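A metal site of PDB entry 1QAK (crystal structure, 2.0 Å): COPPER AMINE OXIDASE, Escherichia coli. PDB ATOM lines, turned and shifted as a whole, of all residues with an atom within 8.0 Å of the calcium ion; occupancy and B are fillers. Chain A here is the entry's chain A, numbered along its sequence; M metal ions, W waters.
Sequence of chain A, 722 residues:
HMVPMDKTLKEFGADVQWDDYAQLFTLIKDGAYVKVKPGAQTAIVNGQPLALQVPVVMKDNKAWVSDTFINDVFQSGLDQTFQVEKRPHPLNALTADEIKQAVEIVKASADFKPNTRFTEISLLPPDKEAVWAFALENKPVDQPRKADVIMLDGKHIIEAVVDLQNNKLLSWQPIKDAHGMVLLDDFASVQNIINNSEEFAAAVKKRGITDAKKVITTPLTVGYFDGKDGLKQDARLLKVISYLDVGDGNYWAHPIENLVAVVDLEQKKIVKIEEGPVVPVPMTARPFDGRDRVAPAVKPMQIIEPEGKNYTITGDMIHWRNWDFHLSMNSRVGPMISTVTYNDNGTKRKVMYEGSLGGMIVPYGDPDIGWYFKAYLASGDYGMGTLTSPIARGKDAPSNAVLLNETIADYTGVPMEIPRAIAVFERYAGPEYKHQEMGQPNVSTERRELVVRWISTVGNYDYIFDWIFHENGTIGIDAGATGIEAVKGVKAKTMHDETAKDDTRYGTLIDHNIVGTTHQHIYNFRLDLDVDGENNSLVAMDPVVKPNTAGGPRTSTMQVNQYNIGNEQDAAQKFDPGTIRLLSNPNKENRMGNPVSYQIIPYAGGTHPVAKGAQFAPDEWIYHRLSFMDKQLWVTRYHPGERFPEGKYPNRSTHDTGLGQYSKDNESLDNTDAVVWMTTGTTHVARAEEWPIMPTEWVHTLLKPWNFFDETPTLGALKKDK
The backbone NH (N) of Arg 637 lies close to the side-chain carboxylate (OE2) of Glu 568, at 2.8 Å.
The backbone NH of Glu 568 sits close to the side-chain amide nitrogen of Asn 666.
ND1 of His 639 sits at hydrogen-bond distance from OE1 of Glu 642 (3.4 Å).
The backbone carbonyl oxygen (O) of Arg 637 sits at hydrogen-bond distance from a ring nitrogen (ND1) of His 639 (3.5 Å).
OE2 of Glu 667 lies within salt-bridge range of NH1 of Arg 637.
Residues that only touch the calcium ion: His 639 (3.99 Å).
The calcium ion is bound by the backbone carbonyl oxygen (O) of Tyr 662 (2.4 Å), the side-chain carboxylate (OE2) of Glu 568 (2.5 Å), water W1 (2.6 Å), the side-chain carboxylate (OE1) of Glu 667 (2.6 Å), the side-chain carboxylate (OD2) of Asp 665 (2.8 Å) and the side-chain carboxylate (OE1) of Glu 568 (2.9 Å).
The calcium ion has six donor atoms within binding distance.
Water W1 lies within hydrogen-bond range of O of Arg 637 (2.5 Å), ND1 of His 639 (2.6 Å) and OE1 of Glu 642 (2.6 Å).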
ATOM      1  N   GLU A 568       2.825   4.405  31.361  1.00  0.00           N
ATOM      2  CA  GLU A 568       2.189   4.403  30.053  1.00  0.00           C
ATOM      3  C   GLU A 568       0.998   5.322  29.899  1.00  0.00           C
ATOM      4  O   GLU A 568       0.893   5.959  28.850  1.00  0.00           O
ATOM      5  CB  GLU A 568       1.881   2.969  29.587  1.00  0.00           C
ATOM      6  CG  GLU A 568       3.082   2.044  29.550  1.00  0.00           C
ATOM      7  CD  GLU A 568       2.738   0.590  29.295  1.00  0.00           C
ATOM      8  OE1 GLU A 568       1.739   0.098  29.854  1.00  0.00           O
ATOM      9  OE2 GLU A 568       3.471  -0.076  28.530  1.00  0.00           O
ATOM     10  N   VAL A 635       4.157   5.872  24.598  1.00  0.00           N
ATOM     11  CA  VAL A 635       5.394   5.193  24.977  1.00  0.00           C
ATOM     12  C   VAL A 635       4.878   3.980  25.762  1.00  0.00           C
ATOM     13  O   VAL A 635       4.079   4.108  26.710  1.00  0.00           O
ATOM     14  CB  VAL A 635       6.400   6.013  25.784  1.00  0.00           C
ATOM     15  CG1 VAL A 635       7.680   5.227  25.985  1.00  0.00           C
ATOM     16  CG2 VAL A 635       6.596   7.354  25.100  1.00  0.00           C
ATOM     17  N   THR A 636       5.289   2.778  25.387  1.00  0.00           N
ATOM     18  CA  THR A 636       4.832   1.564  26.084  1.00  0.00           C
ATOM     19  C   THR A 636       6.089   0.740  26.305  1.00  0.00           C
ATOM     20  O   THR A 636       7.185   0.927  25.735  1.00  0.00           O
ATOM     21  CB  THR A 636       3.893   0.738  25.162  1.00  0.00           C
ATOM     22  OG1 THR A 636       4.649   0.387  23.983  1.00  0.00           O
ATOM     23  CG2 THR A 636       2.676   1.537  24.689  1.00  0.00           C
ATOM     24  N   ARG A 637       5.941  -0.224  27.200  1.00  0.00           N
ATOM     25  CA  ARG A 637       7.053  -1.126  27.539  1.00  0.00           C
ATOM     26  C   ARG A 637       7.261  -2.082  26.356  1.00  0.00           C
ATOM     27  O   ARG A 637       6.266  -2.517  25.787  1.00  0.00           O
ATOM     28  CB  ARG A 637       6.767  -1.927  28.814  1.00  0.00           C
ATOM     29  CG  ARG A 637       7.880  -2.959  28.911  1.00  0.00           C
ATOM     30  CD  ARG A 637       9.202  -2.414  29.480  1.00  0.00           C
ATOM     31  NE  ARG A 637       9.147  -2.472  30.929  1.00  0.00           N
ATOM     32  CZ  ARG A 637       8.243  -2.635  31.889  1.00  0.00           C
ATOM     33  NH1 ARG A 637       6.956  -2.792  31.618  1.00  0.00           N
ATOM     34  NH2 ARG A 637       8.695  -2.606  33.134  1.00  0.00           N
ATOM     35  N   TYR A 638       8.511  -2.378  26.004  1.00  0.00           N
ATOM     36  CA  TYR A 638       8.739  -3.265  24.878  1.00  0.00           C
ATOM     37  C   TYR A 638       8.161  -4.660  25.083  1.00  0.00           C
ATOM     38  O   TYR A 638       8.389  -5.234  26.152  1.00  0.00           O
ATOM     39  CB  TYR A 638      10.239  -3.486  24.678  1.00  0.00           C
ATOM     40  CG  TYR A 638      10.587  -4.575  23.686  1.00  0.00           C
ATOM     41  CD1 TYR A 638      10.447  -4.387  22.320  1.00  0.00           C
ATOM     42  CD2 TYR A 638      11.076  -5.799  24.154  1.00  0.00           C
ATOM     43  CE1 TYR A 638      10.746  -5.381  21.406  1.00  0.00           C
ATOM     44  CE2 TYR A 638      11.375  -6.793  23.240  1.00  0.00           C
ATOM     45  CZ  TYR A 638      11.214  -6.597  21.884  1.00  0.00           C
ATOM     46  OH  TYR A 638      11.539  -7.596  20.990  1.00  0.00           O
ATOM     47  N   HIS A 639       7.482  -5.197  24.100  1.00  0.00           N
ATOM     48  CA  HIS A 639       6.884  -6.548  24.119  1.00  0.00           C
ATOM     49  C   HIS A 639       6.907  -6.935  22.643  1.00  0.00           C
ATOM     50  O   HIS A 639       6.399  -6.261  21.742  1.00  0.00           O
ATOM     51  CB  HIS A 639       5.518  -6.612  24.805  1.00  0.00           C
ATOM     52  CG  HIS A 639       5.479  -6.247  26.261  1.00  0.00           C
ATOM     53  ND1 HIS A 639       4.547  -5.371  26.809  1.00  0.00           N
ATOM     54  CD2 HIS A 639       6.267  -6.614  27.307  1.00  0.00           C
ATOM     55  CE1 HIS A 639       4.760  -5.230  28.115  1.00  0.00           C
ATOM     56  NE2 HIS A 639       5.813  -5.972  28.435  1.00  0.00           N
ATOM     57  N   GLU A 642       3.591  -6.668  20.292  1.00  0.00           N
ATOM     58  CA  GLU A 642       2.807  -5.439  20.312  1.00  0.00           C
ATOM     59  C   GLU A 642       3.435  -4.619  19.186  1.00  0.00           C
ATOM     60  O   GLU A 642       4.375  -3.876  19.393  1.00  0.00           O
ATOM     61  CB  GLU A 642       2.864  -4.675  21.648  1.00  0.00           C
ATOM     62  CG  GLU A 642       2.256  -5.563  22.746  1.00  0.00           C
ATOM     63  CD  GLU A 642       2.233  -4.853  24.078  1.00  0.00           C
ATOM     64  OE1 GLU A 642       2.964  -3.857  24.260  1.00  0.00           O
ATOM     65  OE2 GLU A 642       1.451  -5.295  24.944  1.00  0.00           O
ATOM     66  N   LEU A 659      -2.861   0.088  20.517  1.00  0.00           N
ATOM     67  CA  LEU A 659      -2.270   0.956  21.541  1.00  0.00           C
ATOM     68  C   LEU A 659      -3.185   1.140  22.758  1.00  0.00           C
ATOM     69  O   LEU A 659      -2.648   1.344  23.847  1.00  0.00           O
ATOM     70  CB  LEU A 659      -1.835   2.314  20.955  1.00  0.00           C
ATOM     71  CG  LEU A 659      -0.424   2.281  20.323  1.00  0.00           C
ATOM     72  CD1 LEU A 659      -0.094   3.536  19.522  1.00  0.00           C
ATOM     73  CD2 LEU A 659       0.643   2.105  21.401  1.00  0.00           C
ATOM     74  N   GLY A 660      -4.503   1.078  22.596  1.00  0.00           N
ATOM     75  CA  GLY A 660      -5.368   1.236  23.759  1.00  0.00           C
ATOM     76  C   GLY A 660      -5.088   0.036  24.666  1.00  0.00           C
ATOM     77  O   GLY A 660      -5.023   0.150  25.893  1.00  0.00           O
ATOM     78  N   GLN A 661      -4.905  -1.143  24.073  1.00  0.00           N
ATOM     79  CA  GLN A 661      -4.644  -2.368  24.833  1.00  0.00           C
ATOM     80  C   GLN A 661      -3.214  -2.433  25.362  1.00  0.00           C
ATOM     81  O   GLN A 661      -2.986  -2.886  26.486  1.00  0.00           O
ATOM     82  CB  GLN A 661      -4.855  -3.611  23.957  1.00  0.00           C
ATOM     83  CG  GLN A 661      -4.496  -4.982  24.485  1.00  0.00           C
ATOM     84  CD  GLN A 661      -4.635  -6.093  23.445  1.00  0.00           C
ATOM     85  OE1 GLN A 661      -5.600  -6.449  22.770  1.00  0.00           O
ATOM     86  NE2 GLN A 661      -3.530  -6.784  23.214  1.00  0.00           N
ATOM     87  N   TYR A 662      -2.245  -1.993  24.560  1.00  0.00           N
ATOM     88  CA  TYR A 662      -0.849  -2.036  24.947  1.00  0.00           C
ATOM     89  C   TYR A 662      -0.538  -1.122  26.126  1.00  0.00           C
ATOM     90  O   TYR A 662       0.427  -1.448  26.801  1.00  0.00           O
ATOM     91  CB  TYR A 662       0.120  -1.562  23.822  1.00  0.00           C
ATOM     92  CG  TYR A 662      -0.029  -2.301  22.512  1.00  0.00           C
ATOM     93  CD1 TYR A 662      -0.599  -3.574  22.443  1.00  0.00           C
ATOM     94  CD2 TYR A 662       0.412  -1.750  21.315  1.00  0.00           C
ATOM     95  CE1 TYR A 662      -0.744  -4.264  21.252  1.00  0.00           C
ATOM     96  CE2 TYR A 662       0.272  -2.416  20.107  1.00  0.00           C
ATOM     97  CZ  TYR A 662      -0.290  -3.655  20.092  1.00  0.00           C
ATOM     98  OH  TYR A 662      -0.434  -4.338  18.906  1.00  0.00           O
ATOM     99  N   SER A 663      -1.295  -0.070  26.324  1.00  0.00           N
ATOM    100  CA  SER A 663      -1.038   0.829  27.445  1.00  0.00           C
ATOM    101  C   SER A 663      -2.046   0.704  28.581  1.00  0.00           C
ATOM    102  O   SER A 663      -1.838   1.303  29.637  1.00  0.00           O
ATOM    103  CB  SER A 663      -1.083   2.260  26.885  1.00  0.00           C
ATOM    104  OG  SER A 663      -2.396   2.591  26.409  1.00  0.00           O
ATOM    105  N   LYS A 664      -3.116  -0.051  28.356  1.00  0.00           N
ATOM    106  CA  LYS A 664      -4.195  -0.281  29.309  1.00  0.00           C
ATOM    107  C   LYS A 664      -3.719  -0.582  30.733  1.00  0.00           C
ATOM    108  O   LYS A 664      -4.259  -0.044  31.676  1.00  0.00           O
ATOM    109  CB  LYS A 664      -5.031  -1.502  28.856  1.00  0.00           C
ATOM    110  CG  LYS A 664      -6.507  -1.323  29.190  1.00  0.00           C
ATOM    111  CD  LYS A 664      -7.393  -2.473  28.699  1.00  0.00           C
ATOM    112  CE  LYS A 664      -8.556  -2.698  29.638  1.00  0.00           C
ATOM    113  NZ  LYS A 664      -8.130  -3.170  30.996  1.00  0.00           N
ATOM    114  N   ASP A 665      -2.730  -1.435  30.858  1.00  0.00           N
ATOM    115  CA  ASP A 665      -2.108  -1.879  32.089  1.00  0.00           C
ATOM    116  C   ASP A 665      -1.328  -0.754  32.755  1.00  0.00           C
ATOM    117  O   ASP A 665      -0.893  -0.945  33.876  1.00  0.00           O
ATOM    118  CB  ASP A 665      -1.145  -3.028  31.745  1.00  0.00           C
ATOM    119  CG  ASP A 665      -0.281  -2.679  30.531  1.00  0.00           C
ATOM    120  OD1 ASP A 665      -0.597  -1.802  29.688  1.00  0.00           O
ATOM    121  OD2 ASP A 665       0.802  -3.295  30.352  1.00  0.00           O
ATOM    122  N   ASN A 666      -1.158   0.380  32.080  1.00  0.00           N
ATOM    123  CA  ASN A 666      -0.443   1.503  32.658  1.00  0.00           C
ATOM    124  C   ASN A 666       0.824   1.119  33.390  1.00  0.00           C
ATOM    125  O   ASN A 666       0.968   1.438  34.572  1.00  0.00           O
ATOM    126  CB  ASN A 666      -1.315   2.255  33.674  1.00  0.00           C
ATOM    127  CG  ASN A 666      -0.780   3.594  34.089  1.00  0.00           C
ATOM    128  OD1 ASN A 666      -1.326   4.190  35.039  1.00  0.00           O
ATOM    129  ND2 ASN A 666       0.255   4.098  33.394  1.00  0.00           N
ATOM    130  N   GLU A 667       1.735   0.447  32.711  1.00  0.00           N
ATOM    131  CA  GLU A 667       2.982   0.017  33.341  1.00  0.00           C
ATOM    132  C   GLU A 667       3.987   1.163  33.460  1.00  0.00           C
ATOM    133  O   GLU A 667       3.881   2.229  32.857  1.00  0.00           O
ATOM    134  CB  GLU A 667       3.563  -1.140  32.526  1.00  0.00           C
ATOM    135  CG  GLU A 667       2.710  -2.387  32.372  1.00  0.00           C
ATOM    136  CD  GLU A 667       3.419  -3.412  31.486  1.00  0.00           C
ATOM    137  OE1 GLU A 667       3.293  -3.421  30.244  1.00  0.00           O
ATOM    138  OE2 GLU A 667       4.168  -4.239  32.081  1.00  0.00           O
ATOM    139  N   SER A 668       5.006   0.935  34.265  1.00  0.00           N
ATOM    140  CA  SER A 668       6.090   1.825  34.577  1.00  0.00           C
ATOM    141  C   SER A 668       7.060   1.912  33.395  1.00  0.00           C
ATOM    142  O   SER A 668       7.409   0.925  32.730  1.00  0.00           O
ATOM    143  CB  SER A 668       6.918   1.171  35.712  1.00  0.00           C
ATOM    144  OG  SER A 668       8.095   1.937  35.879  1.00  0.00           O
ATOM    145  N   LEU A 669       7.466   3.149  33.152  1.00  0.00           N
ATOM    146  CA  LEU A 669       8.375   3.456  32.068  1.00  0.00           C
ATOM    147  C   LEU A 669       9.650   4.007  32.685  1.00  0.00           C
ATOM    148  O   LEU A 669      10.371   4.693  31.971  1.00  0.00           O
ATOM    149  CB  LEU A 669       7.767   4.531  31.150  1.00  0.00           C
ATOM    150  CG  LEU A 669       6.561   4.118  30.329  1.00  0.00           C
ATOM    151  CD1 LEU A 669       6.108   5.275  29.433  1.00  0.00           C
ATOM    152  CD2 LEU A 669       6.881   2.913  29.458  1.00  0.00           C
HETATM  153 CA    CA M   1       2.169  -2.202  28.224  1.00  0.00          CA
HETATM  154  O   HOH W   1       3.903  -2.918  26.485  1.00  0.00           O
